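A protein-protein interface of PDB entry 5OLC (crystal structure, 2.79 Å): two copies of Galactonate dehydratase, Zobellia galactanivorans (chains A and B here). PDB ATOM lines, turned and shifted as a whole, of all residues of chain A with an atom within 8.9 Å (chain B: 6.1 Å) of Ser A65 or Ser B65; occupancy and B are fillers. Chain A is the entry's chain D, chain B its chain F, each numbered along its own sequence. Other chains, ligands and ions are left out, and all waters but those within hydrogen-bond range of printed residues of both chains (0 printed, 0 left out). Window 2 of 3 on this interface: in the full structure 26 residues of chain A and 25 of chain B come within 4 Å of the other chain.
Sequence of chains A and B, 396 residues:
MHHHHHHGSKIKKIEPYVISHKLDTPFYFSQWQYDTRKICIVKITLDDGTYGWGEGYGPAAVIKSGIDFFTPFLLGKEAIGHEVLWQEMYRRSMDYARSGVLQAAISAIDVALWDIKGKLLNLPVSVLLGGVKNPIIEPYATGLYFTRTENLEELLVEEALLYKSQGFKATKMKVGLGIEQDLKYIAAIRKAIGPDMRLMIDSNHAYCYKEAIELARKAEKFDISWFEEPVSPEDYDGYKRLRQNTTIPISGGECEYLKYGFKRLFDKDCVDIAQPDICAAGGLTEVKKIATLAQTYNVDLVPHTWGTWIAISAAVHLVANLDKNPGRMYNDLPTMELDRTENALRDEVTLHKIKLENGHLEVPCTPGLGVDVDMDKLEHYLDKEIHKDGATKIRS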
ATOM      1  N   PRO A  16     -11.139  -2.080 -17.813  1.00  0.00           N
ATOM      2  CA  PRO A  16      -9.942  -2.473 -18.586  1.00  0.00           C
ATOM      3  C   PRO A  16      -8.742  -1.541 -18.374  1.00  0.00           C
ATOM      4  O   PRO A  16      -8.922  -0.330 -18.280  1.00  0.00           O
ATOM      5  CB  PRO A  16     -10.440  -2.469 -20.023  1.00  0.00           C
ATOM      6  CG  PRO A  16     -11.562  -1.473 -20.043  1.00  0.00           C
ATOM      7  CD  PRO A  16     -12.120  -1.356 -18.658  1.00  0.00           C
ATOM      8  N   TYR A  17      -7.525  -2.106 -18.278  1.00  0.00           N
ATOM      9  CA  TYR A  17      -6.300  -1.350 -18.009  1.00  0.00           C
ATOM     10  C   TYR A  17      -5.135  -1.695 -18.953  1.00  0.00           C
ATOM     11  O   TYR A  17      -4.543  -2.776 -18.835  1.00  0.00           O
ATOM     12  CB  TYR A  17      -5.833  -1.529 -16.531  1.00  0.00           C
ATOM     13  CG  TYR A  17      -6.857  -1.242 -15.442  1.00  0.00           C
ATOM     14  CD1 TYR A  17      -7.262   0.064 -15.161  1.00  0.00           C
ATOM     15  CD2 TYR A  17      -7.351  -2.263 -14.630  1.00  0.00           C
ATOM     16  CE1 TYR A  17      -8.179   0.341 -14.142  1.00  0.00           C
ATOM     17  CE2 TYR A  17      -8.276  -1.998 -13.613  1.00  0.00           C
ATOM     18  CZ  TYR A  17      -8.679  -0.692 -13.368  1.00  0.00           C
ATOM     19  OH  TYR A  17      -9.586  -0.402 -12.379  1.00  0.00           O
ATOM     20  N   VAL A  18      -4.779  -0.760 -19.866  1.00  0.00           N
ATOM     21  CA  VAL A  18      -3.625  -0.911 -20.766  1.00  0.00           C
ATOM     22  C   VAL A  18      -2.383  -0.450 -19.990  1.00  0.00           C
ATOM     23  O   VAL A  18      -2.330   0.698 -19.528  1.00  0.00           O
ATOM     24  CB  VAL A  18      -3.802  -0.156 -22.100  1.00  0.00           C
ATOM     25  CG1 VAL A  18      -2.500  -0.134 -22.898  1.00  0.00           C
ATOM     26  CG2 VAL A  18      -4.911  -0.780 -22.915  1.00  0.00           C
ATOM     27  N   CYS A  40      -3.185  -5.627 -22.251  1.00  0.00           N
ATOM     28  CA  CYS A  40      -4.426  -5.145 -21.630  1.00  0.00           C
ATOM     29  C   CYS A  40      -4.830  -6.150 -20.546  1.00  0.00           C
ATOM     30  O   CYS A  40      -4.428  -7.312 -20.605  1.00  0.00           O
ATOM     31  CB  CYS A  40      -5.529  -4.943 -22.666  1.00  0.00           C
ATOM     32  SG  CYS A  40      -7.146  -4.500 -21.971  1.00  0.00           S
ATOM     33  N   PRO A  59      -3.065  -6.918 -29.358  1.00  0.00           N
ATOM     34  CA  PRO A  59      -2.787  -5.469 -29.248  1.00  0.00           C
ATOM     35  C   PRO A  59      -3.636  -4.792 -28.168  1.00  0.00           C
ATOM     36  O   PRO A  59      -4.840  -4.530 -28.342  1.00  0.00           O
ATOM     37  CB  PRO A  59      -3.036  -4.937 -30.673  1.00  0.00           C
ATOM     38  CG  PRO A  59      -3.533  -6.127 -31.485  1.00  0.00           C
ATOM     39  CD  PRO A  59      -3.945  -7.191 -30.509  1.00  0.00           C
ATOM     40  N   ALA A  60      -2.974  -4.521 -27.029  1.00  0.00           N
ATOM     41  CA  ALA A  60      -3.554  -3.952 -25.818  1.00  0.00           C
ATOM     42  C   ALA A  60      -4.725  -2.963 -26.048  1.00  0.00           C
ATOM     43  O   ALA A  60      -5.865  -3.298 -25.738  1.00  0.00           O
ATOM     44  CB  ALA A  60      -2.470  -3.319 -24.964  1.00  0.00           C
ATOM     45  N   ALA A  61      -4.448  -1.788 -26.624  1.00  0.00           N
ATOM     46  CA  ALA A  61      -5.420  -0.713 -26.839  1.00  0.00           C
ATOM     47  C   ALA A  61      -6.638  -1.093 -27.698  1.00  0.00           C
ATOM     48  O   ALA A  61      -7.699  -0.457 -27.573  1.00  0.00           O
ATOM     49  CB  ALA A  61      -4.721   0.496 -27.421  1.00  0.00           C
ATOM     50  N   VAL A  62      -6.478  -2.135 -28.560  1.00  0.00           N
ATOM     51  CA  VAL A  62      -7.536  -2.641 -29.437  1.00  0.00           C
ATOM     52  C   VAL A  62      -8.424  -3.575 -28.648  1.00  0.00           C
ATOM     53  O   VAL A  62      -9.641  -3.567 -28.850  1.00  0.00           O
ATOM     54  CB  VAL A  62      -7.012  -3.307 -30.724  1.00  0.00           C
ATOM     55  CG1 VAL A  62      -8.031  -3.157 -31.855  1.00  0.00           C
ATOM     56  CG2 VAL A  62      -5.657  -2.732 -31.133  1.00  0.00           C
ATOM     57  N   ILE A  63      -7.820  -4.383 -27.745  1.00  0.00           N
ATOM     58  CA  ILE A  63      -8.564  -5.299 -26.857  1.00  0.00           C
ATOM     59  C   ILE A  63      -9.376  -4.431 -25.857  1.00  0.00           C
ATOM     60  O   ILE A  63     -10.543  -4.707 -25.589  1.00  0.00           O
ATOM     61  CB  ILE A  63      -7.604  -6.312 -26.116  1.00  0.00           C
ATOM     62  CG1 ILE A  63      -6.837  -7.222 -27.100  1.00  0.00           C
ATOM     63  CG2 ILE A  63      -8.325  -7.147 -25.028  1.00  0.00           C
ATOM     64  CD1 ILE A  63      -5.436  -7.581 -26.601  1.00  0.00           C
ATOM     65  N   LYS A  64      -8.735  -3.376 -25.339  1.00  0.00           N
ATOM     66  CA  LYS A  64      -9.288  -2.466 -24.358  1.00  0.00           C
ATOM     67  C   LYS A  64     -10.588  -1.830 -24.860  1.00  0.00           C
ATOM     68  O   LYS A  64     -11.518  -1.619 -24.079  1.00  0.00           O
ATOM     69  CB  LYS A  64      -8.251  -1.401 -24.005  1.00  0.00           C
ATOM     70  CG  LYS A  64      -8.460  -0.775 -22.635  1.00  0.00           C
ATOM     71  CD  LYS A  64      -8.692   0.711 -22.722  1.00  0.00           C
ATOM     72  CE  LYS A  64     -10.135   1.095 -22.512  1.00  0.00           C
ATOM     73  NZ  LYS A  64     -10.356   2.536 -22.831  1.00  0.00           N
ATOM     74  N   SER A  65     -10.664  -1.553 -26.153  1.00  0.00           N
ATOM     75  CA  SER A  65     -11.861  -0.958 -26.741  1.00  0.00           C
ATOM     76  C   SER A  65     -12.915  -2.020 -26.909  1.00  0.00           C
ATOM     77  O   SER A  65     -14.109  -1.706 -26.870  1.00  0.00           O
ATOM     78  CB  SER A  65     -11.534  -0.316 -28.086  1.00  0.00           C
ATOM     79  OG  SER A  65     -10.573   0.701 -27.900  1.00  0.00           O
ATOM     80  N   GLY A  66     -12.445  -3.258 -27.124  1.00  0.00           N
ATOM     81  CA  GLY A  66     -13.271  -4.444 -27.293  1.00  0.00           C
ATOM     82  C   GLY A  66     -14.075  -4.671 -26.037  1.00  0.00           C
ATOM     83  O   GLY A  66     -15.298  -4.766 -26.116  1.00  0.00           O
ATOM     84  N   ILE A  67     -13.395  -4.676 -24.858  1.00  0.00           N
ATOM     85  CA  ILE A  67     -14.020  -4.831 -23.536  1.00  0.00           C
ATOM     86  C   ILE A  67     -15.101  -3.754 -23.375  1.00  0.00           C
ATOM     87  O   ILE A  67     -16.237  -4.095 -23.027  1.00  0.00           O
ATOM     88  CB  ILE A  67     -12.978  -4.800 -22.400  1.00  0.00           C
ATOM     89  CG1 ILE A  67     -12.101  -6.057 -22.425  1.00  0.00           C
ATOM     90  CG2 ILE A  67     -13.676  -4.656 -21.061  1.00  0.00           C
ATOM     91  CD1 ILE A  67     -10.660  -5.851 -22.120  1.00  0.00           C
ATOM     92  N   ASP A  68     -14.759  -2.476 -23.715  1.00  0.00           N
ATOM     93  CA  ASP A  68     -15.664  -1.327 -23.699  1.00  0.00           C
ATOM     94  C   ASP A  68     -16.915  -1.559 -24.578  1.00  0.00           C
ATOM     95  O   ASP A  68     -17.984  -1.005 -24.280  1.00  0.00           O
ATOM     96  CB  ASP A  68     -14.941  -0.071 -24.196  1.00  0.00           C
ATOM     97  CG  ASP A  68     -13.808   0.483 -23.347  1.00  0.00           C
ATOM     98  OD1 ASP A  68     -13.584  -0.039 -22.236  1.00  0.00           O
ATOM     99  OD2 ASP A  68     -13.166   1.465 -23.785  1.00  0.00           O
ATOM    100  N   PHE A  69     -16.768  -2.356 -25.672  1.00  0.00           N
ATOM    101  CA  PHE A  69     -17.863  -2.679 -26.578  1.00  0.00           C
ATOM    102  C   PHE A  69     -18.896  -3.577 -25.895  1.00  0.00           C
ATOM    103  O   PHE A  69     -20.093  -3.320 -26.021  1.00  0.00           O
ATOM    104  CB  PHE A  69     -17.354  -3.303 -27.901  1.00  0.00           C
ATOM    105  CG  PHE A  69     -18.452  -3.868 -28.781  1.00  0.00           C
ATOM    106  CD1 PHE A  69     -19.256  -3.030 -29.547  1.00  0.00           C
ATOM    107  CD2 PHE A  69     -18.706  -5.231 -28.816  1.00  0.00           C
ATOM    108  CE1 PHE A  69     -20.290  -3.547 -30.324  1.00  0.00           C
ATOM    109  CE2 PHE A  69     -19.744  -5.745 -29.595  1.00  0.00           C
ATOM    110  CZ  PHE A  69     -20.522  -4.902 -30.349  1.00  0.00           C
ATOM    111  N   PHE A  70     -18.433  -4.615 -25.181  1.00  0.00           N
ATOM    112  CA  PHE A  70     -19.300  -5.558 -24.479  1.00  0.00           C
ATOM    113  C   PHE A  70     -19.785  -5.066 -23.126  1.00  0.00           C
ATOM    114  O   PHE A  70     -20.773  -5.610 -22.610  1.00  0.00           O
ATOM    115  CB  PHE A  70     -18.582  -6.904 -24.266  1.00  0.00           C
ATOM    116  CG  PHE A  70     -18.112  -7.582 -25.528  1.00  0.00           C
ATOM    117  CD1 PHE A  70     -19.027  -8.020 -26.485  1.00  0.00           C
ATOM    118  CD2 PHE A  70     -16.758  -7.813 -25.745  1.00  0.00           C
ATOM    119  CE1 PHE A  70     -18.593  -8.639 -27.648  1.00  0.00           C
ATOM    120  CE2 PHE A  70     -16.321  -8.429 -26.911  1.00  0.00           C
ATOM    121  CZ  PHE A  70     -17.242  -8.844 -27.853  1.00  0.00           C
ATOM    122  N   THR A  71     -19.064  -4.088 -22.523  1.00  0.00           N
ATOM    123  CA  THR A  71     -19.356  -3.609 -21.179  1.00  0.00           C
ATOM    124  C   THR A  71     -20.831  -3.205 -21.060  1.00  0.00           C
ATOM    125  O   THR A  71     -21.448  -3.755 -20.153  1.00  0.00           O
ATOM    126  CB  THR A  71     -18.340  -2.567 -20.703  1.00  0.00           C
ATOM    127  OG1 THR A  71     -17.054  -3.188 -20.670  1.00  0.00           O
ATOM    128  CG2 THR A  71     -18.635  -2.055 -19.308  1.00  0.00           C
ATOM    129  N   PRO A  72     -21.470  -2.425 -21.976  1.00  0.00           N
ATOM    130  CA  PRO A  72     -22.906  -2.108 -21.795  1.00  0.00           C
ATOM    131  C   PRO A  72     -23.854  -3.296 -21.581  1.00  0.00           C
ATOM    132  O   PRO A  72     -24.757  -3.171 -20.753  1.00  0.00           O
ATOM    133  CB  PRO A  72     -23.266  -1.333 -23.066  1.00  0.00           C
ATOM    134  CG  PRO A  72     -22.006  -0.697 -23.468  1.00  0.00           C
ATOM    135  CD  PRO A  72     -20.920  -1.689 -23.134  1.00  0.00           C
ATOM    136  N   VAL A 101      -8.939  -9.841 -32.222  1.00  0.00           N
ATOM    137  CA  VAL A 101      -9.202  -8.786 -31.247  1.00  0.00           C
ATOM    138  C   VAL A 101     -10.477  -9.008 -30.404  1.00  0.00           C
ATOM    139  O   VAL A 101     -10.326  -9.119 -29.189  1.00  0.00           O
ATOM    140  CB  VAL A 101      -9.167  -7.387 -31.938  1.00  0.00           C
ATOM    141  CG1 VAL A 101      -9.810  -6.295 -31.082  1.00  0.00           C
ATOM    142  CG2 VAL A 101      -7.738  -7.001 -32.297  1.00  0.00           C
ATOM    143  N   LEU A 102     -11.702  -9.061 -30.991  1.00  0.00           N
ATOM    144  CA  LEU A 102     -12.909  -9.246 -30.164  1.00  0.00           C
ATOM    145  C   LEU A 102     -12.911 -10.576 -29.379  1.00  0.00           C
ATOM    146  O   LEU A 102     -13.549 -10.646 -28.330  1.00  0.00           O
ATOM    147  CB  LEU A 102     -14.215  -9.052 -30.938  1.00  0.00           C
ATOM    148  CG  LEU A 102     -14.624  -7.607 -31.236  1.00  0.00           C
ATOM    149  CD1 LEU A 102     -15.759  -7.560 -32.233  1.00  0.00           C
ATOM    150  CD2 LEU A 102     -15.051  -6.861 -29.988  1.00  0.00           C
ATOM    151  N   ALA A 105     -10.991  -9.848 -26.273  1.00  0.00           N
ATOM    152  CA  ALA A 105     -11.873  -9.047 -25.406  1.00  0.00           C
ATOM    153  C   ALA A 105     -12.811 -10.009 -24.659  1.00  0.00           C
ATOM    154  O   ALA A 105     -12.980  -9.845 -23.444  1.00  0.00           O
ATOM    155  CB  ALA A 105     -12.692  -8.059 -26.221  1.00  0.00           C
ATOM    156  N   ILE A 109     -12.645 -10.965 -20.355  1.00  0.00           N
ATOM    157  CA  ILE A 109     -13.840 -10.977 -19.499  1.00  0.00           C
ATOM    158  C   ILE A 109     -14.041 -12.387 -18.900  1.00  0.00           C
ATOM    159  O   ILE A 109     -14.240 -12.509 -17.698  1.00  0.00           O
ATOM    160  CB  ILE A 109     -15.096 -10.464 -20.265  1.00  0.00           C
ATOM    161  CG1 ILE A 109     -14.956  -8.946 -20.603  1.00  0.00           C
ATOM    162  CG2 ILE A 109     -16.404 -10.750 -19.480  1.00  0.00           C
ATOM    163  CD1 ILE A 109     -15.611  -8.503 -21.884  1.00  0.00           C
ATOM    164  N   CYS B  40     -16.826   3.994 -38.196  1.00  0.00           N
ATOM    165  CA  CYS B  40     -15.460   4.506 -38.174  1.00  0.00           C
ATOM    166  C   CYS B  40     -15.043   4.858 -39.618  1.00  0.00           C
ATOM    167  O   CYS B  40     -15.260   4.062 -40.526  1.00  0.00           O
ATOM    168  CB  CYS B  40     -14.492   3.532 -37.523  1.00  0.00           C
ATOM    169  SG  CYS B  40     -12.792   4.154 -37.417  1.00  0.00           S
ATOM    170  N   ALA B  60     -17.355   0.527 -34.588  1.00  0.00           N
ATOM    171  CA  ALA B  60     -16.669   1.807 -34.824  1.00  0.00           C
ATOM    172  C   ALA B  60     -15.424   2.051 -33.977  1.00  0.00           C
ATOM    173  O   ALA B  60     -14.323   2.060 -34.535  1.00  0.00           O
ATOM    174  CB  ALA B  60     -17.627   2.967 -34.688  1.00  0.00           C
ATOM    175  N   ALA B  61     -15.586   2.184 -32.640  1.00  0.00           N
ATOM    176  CA  ALA B  61     -14.523   2.482 -31.680  1.00  0.00           C
ATOM    177  C   ALA B  61     -13.391   1.443 -31.604  1.00  0.00           C
ATOM    178  O   ALA B  61     -12.265   1.783 -31.231  1.00  0.00           O
ATOM    179  CB  ALA B  61     -15.125   2.705 -30.322  1.00  0.00           C
ATOM    180  N   VAL B  62     -13.691   0.183 -31.983  1.00  0.00           N
ATOM    181  CA  VAL B  62     -12.730  -0.929 -31.998  1.00  0.00           C
ATOM    182  C   VAL B  62     -11.902  -0.844 -33.260  1.00  0.00           C
ATOM    183  O   VAL B  62     -10.693  -1.112 -33.229  1.00  0.00           O
ATOM    184  CB  VAL B  62     -13.375  -2.327 -31.831  1.00  0.00           C
ATOM    185  CG1 VAL B  62     -12.405  -3.274 -31.133  1.00  0.00           C
ATOM    186  CG2 VAL B  62     -14.675  -2.245 -31.044  1.00  0.00           C
ATOM    187  N   ILE B  63     -12.553  -0.453 -34.364  1.00  0.00           N
ATOM    188  CA  ILE B  63     -11.895  -0.276 -35.661  1.00  0.00           C
ATOM    189  C   ILE B  63     -10.946   0.940 -35.607  1.00  0.00           C
ATOM    190  O   ILE B  63      -9.826   0.893 -36.149  1.00  0.00           O
ATOM    191  CB  ILE B  63     -12.953  -0.215 -36.820  1.00  0.00           C
ATOM    192  CG1 ILE B  63     -13.529  -1.623 -37.072  1.00  0.00           C
ATOM    193  CG2 ILE B  63     -12.368   0.363 -38.124  1.00  0.00           C
ATOM    194  CD1 ILE B  63     -14.885  -1.634 -37.497  1.00  0.00           C
ATOM    195  N   LYS B  64     -11.411   2.004 -34.914  1.00  0.00           N
ATOM    196  CA  LYS B  64     -10.715   3.264 -34.731  1.00  0.00           C
ATOM    197  C   LYS B  64      -9.391   3.051 -34.012  1.00  0.00           C
ATOM    198  O   LYS B  64      -8.406   3.711 -34.341  1.00  0.00           O
ATOM    199  CB  LYS B  64     -11.612   4.222 -33.952  1.00  0.00           C
ATOM    200  CG  LYS B  64     -11.288   5.685 -34.185  1.00  0.00           C
ATOM    201  CD  LYS B  64     -10.904   6.377 -32.913  1.00  0.00           C
ATOM    202  CE  LYS B  64      -9.415   6.636 -32.827  1.00  0.00           C
ATOM    203  NZ  LYS B  64      -9.025   7.169 -31.499  1.00  0.00           N
ATOM    204  N   SER B  65      -9.359   2.116 -33.057  1.00  0.00           N
ATOM    205  CA  SER B  65      -8.139   1.803 -32.324  1.00  0.00           C
ATOM    206  C   SER B  65      -7.205   0.970 -33.189  1.00  0.00           C
ATOM    207  O   SER B  65      -5.976   1.040 -33.021  1.00  0.00           O
ATOM    208  CB  SER B  65      -8.473   1.058 -31.045  1.00  0.00           C
ATOM    209  OG  SER B  65      -9.284   1.903 -30.255  1.00  0.00           O
ATOM    210  N   GLY B  66      -7.812   0.186 -34.091  1.00  0.00           N
ATOM    211  CA  GLY B  66      -7.103  -0.663 -35.035  1.00  0.00           C
ATOM    212  C   GLY B  66      -6.252   0.184 -35.952  1.00  0.00           C
ATOM    213  O   GLY B  66      -5.037  -0.043 -36.072  1.00  0.00           O
ATOM    214  N   ILE B  67      -6.881   1.224 -36.552  1.00  0.00           N
ATOM    215  CA  ILE B  67      -6.202   2.177 -37.438  1.00  0.00           C
ATOM    216  C   ILE B  67      -5.018   2.795 -36.686  1.00  0.00           C
ATOM    217  O   ILE B  67      -3.910   2.808 -37.215  1.00  0.00           O
ATOM    218  CB  ILE B  67      -7.182   3.236 -37.986  1.00  0.00           C
ATOM    219  CG1 ILE B  67      -8.175   2.607 -38.984  1.00  0.00           C
ATOM    220  CG2 ILE B  67      -6.416   4.374 -38.627  1.00  0.00           C
ATOM    221  CD1 ILE B  67      -9.573   3.088 -38.876  1.00  0.00           C
ATOM    222  N   ASP B  68      -5.249   3.219 -35.420  1.00  0.00           N
ATOM    223  CA  ASP B  68      -4.235   3.779 -34.524  1.00  0.00           C
ATOM    224  C   ASP B  68      -3.062   2.820 -34.323  1.00  0.00           C
ATOM    225  O   ASP B  68      -1.941   3.272 -34.104  1.00  0.00           O
ATOM    226  CB  ASP B  68      -4.846   4.107 -33.153  1.00  0.00           C
ATOM    227  CG  ASP B  68      -5.880   5.215 -33.083  1.00  0.00           C
ATOM    228  OD1 ASP B  68      -6.100   5.893 -34.106  1.00  0.00           O
ATOM    229  OD2 ASP B  68      -6.451   5.422 -31.989  1.00  0.00           O
ATOM    230  N   PHE B  69      -3.333   1.505 -34.369  1.00  0.00           N
ATOM    231  CA  PHE B  69      -2.311   0.474 -34.202  1.00  0.00           C
ATOM    232  C   PHE B  69      -1.342   0.485 -35.382  1.00  0.00           C
ATOM    233  O   PHE B  69      -0.138   0.423 -35.154  1.00  0.00           O
ATOM    234  CB  PHE B  69      -2.920  -0.935 -33.972  1.00  0.00           C
ATOM    235  CG  PHE B  69      -1.898  -2.052 -34.038  1.00  0.00           C
ATOM    236  CD1 PHE B  69      -1.045  -2.305 -32.969  1.00  0.00           C
ATOM    237  CD2 PHE B  69      -1.771  -2.836 -35.178  1.00  0.00           C
ATOM    238  CE1 PHE B  69      -0.090  -3.331 -33.035  1.00  0.00           C
ATOM    239  CE2 PHE B  69      -0.804  -3.853 -35.248  1.00  0.00           C
ATOM    240  CZ  PHE B  69       0.026  -4.095 -34.175  1.00  0.00           C
ATOM    241  N   PHE B  70      -1.863   0.565 -36.619  1.00  0.00           N
ATOM    242  CA  PHE B  70      -1.054   0.557 -37.844  1.00  0.00           C
ATOM    243  C   PHE B  70      -0.467   1.898 -38.206  1.00  0.00           C
ATOM    244  O   PHE B  70       0.492   1.947 -38.989  1.00  0.00           O
ATOM    245  CB  PHE B  70      -1.860   0.051 -39.052  1.00  0.00           C
ATOM    246  CG  PHE B  70      -2.448  -1.326 -38.897  1.00  0.00           C
ATOM    247  CD1 PHE B  70      -1.622  -2.444 -38.788  1.00  0.00           C
ATOM    248  CD2 PHE B  70      -3.831  -1.511 -38.880  1.00  0.00           C
ATOM    249  CE1 PHE B  70      -2.165  -3.715 -38.631  1.00  0.00           C
ATOM    250  CE2 PHE B  70      -4.377  -2.785 -38.726  1.00  0.00           C
ATOM    251  CZ  PHE B  70      -3.543  -3.880 -38.607  1.00  0.00           C
ATOM    252  N   LEU B 102      -9.227  -6.147 -36.738  1.00  0.00           N
ATOM    253  CA  LEU B 102      -8.020  -5.629 -37.414  1.00  0.00           C
ATOM    254  C   LEU B 102      -8.101  -5.672 -38.958  1.00  0.00           C
ATOM    255  O   LEU B 102      -7.412  -4.898 -39.622  1.00  0.00           O
ATOM    256  CB  LEU B 102      -6.727  -6.278 -36.914  1.00  0.00           C
ATOM    257  CG  LEU B 102      -6.177  -5.786 -35.590  1.00  0.00           C
ATOM    258  CD1 LEU B 102      -5.094  -6.686 -35.102  1.00  0.00           C
ATOM    259  CD2 LEU B 102      -5.620  -4.388 -35.693  1.00  0.00           C
ATOM    260  N   ALA B 105      -9.787  -2.520 -39.890  1.00  0.00           N
ATOM    261  CA  ALA B 105      -8.750  -1.500 -39.753  1.00  0.00           C
ATOM    262  C   ALA B 105      -7.882  -1.466 -41.022  1.00  0.00           C
ATOM    263  O   ALA B 105      -7.673  -0.385 -41.563  1.00  0.00           O
ATOM    264  CB  ALA B 105      -7.895  -1.782 -38.534  1.00  0.00           C
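OG of Ser B65 lies within hydrogen-bond range of OG of Ser A65, at 2.9 Å.
The backbone carbonyl oxygen (O) of Ala A61 is in hydrogen-bond range of the side-chain hydroxyl (OG) of Ser A65 (3.1 Å).
O of Ala B61 lies within hydrogen-bond range of OG of Ser B65 (3.1 Å).
Leu B102 touches Pro A59 (CD1 to CG, 3.98 Å).
Ser B65 touches Ala A61 (CB to O, 3.9 Å).
CG1 of Val B62 touches O of Val A62, at 3.6 Å.
Ala B61 touches Ser A65 (O to CB, 3.9 Å).
CG1 of Val B62 touches CG1 of Val A101, at 3.98 Å.
CG of Leu B102 touches CG2 of Val A101, 3.8 Å away.
Cys A40 touches none of the printed residues of chain B.
Ile A63 touches none of the printed residues of chain B.
Of chain B, only Ala B61 and Ser B65 come within 4 Å of Ser A65.
Printed residues of chain B within 4 Å of Val A101: Val B62 and Leu B102.
Of the printed residues of chain A, Ala B61 touches Ser A65 (3.9 Å).
Of the printed residues of chain A, Val B62 touches Val A62 (3.6 Å) and Val A101 (3.98 Å).
Ser B65 touches just these residues of chain A: Ala A61 and Ser A65.
The nearest residue of chain B that does not touch Ser A65 is Val B62 (4.1 Å).
The nearest residue of chain A that does not touch Ser B65 is Val A62 (4.1 Å).
The nearest printed residue of chain A that does not touch Leu B102 is Val A62 (4.7 Å).
Hydrophobic or aromatic side chains of chain B within 4 Å of the printed part of chain A: Val B62 and Leu B102.
Along chain B the printed residues that touch a printed residue of chain A span positions 61 to 102.
Hydrophobic or aromatic side chains of chain A that line the printed part of chain B: Pro A59, Val A62 and Val A101.
Among the printed residues, 7 pairs touch across the chains.
Ala A61 touches Ser B65, and with the chains exchanged Ser A65 touches Ala B61.
Val A62 touches its own counterpart, Val B62.
Ser B65 touches its own counterpart, Ser A65.
14 positions are printed for both chains.
Of the 7 pairs that touch across the chains among the printed residues, 4 have their exchanged pair printed and touching as well.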
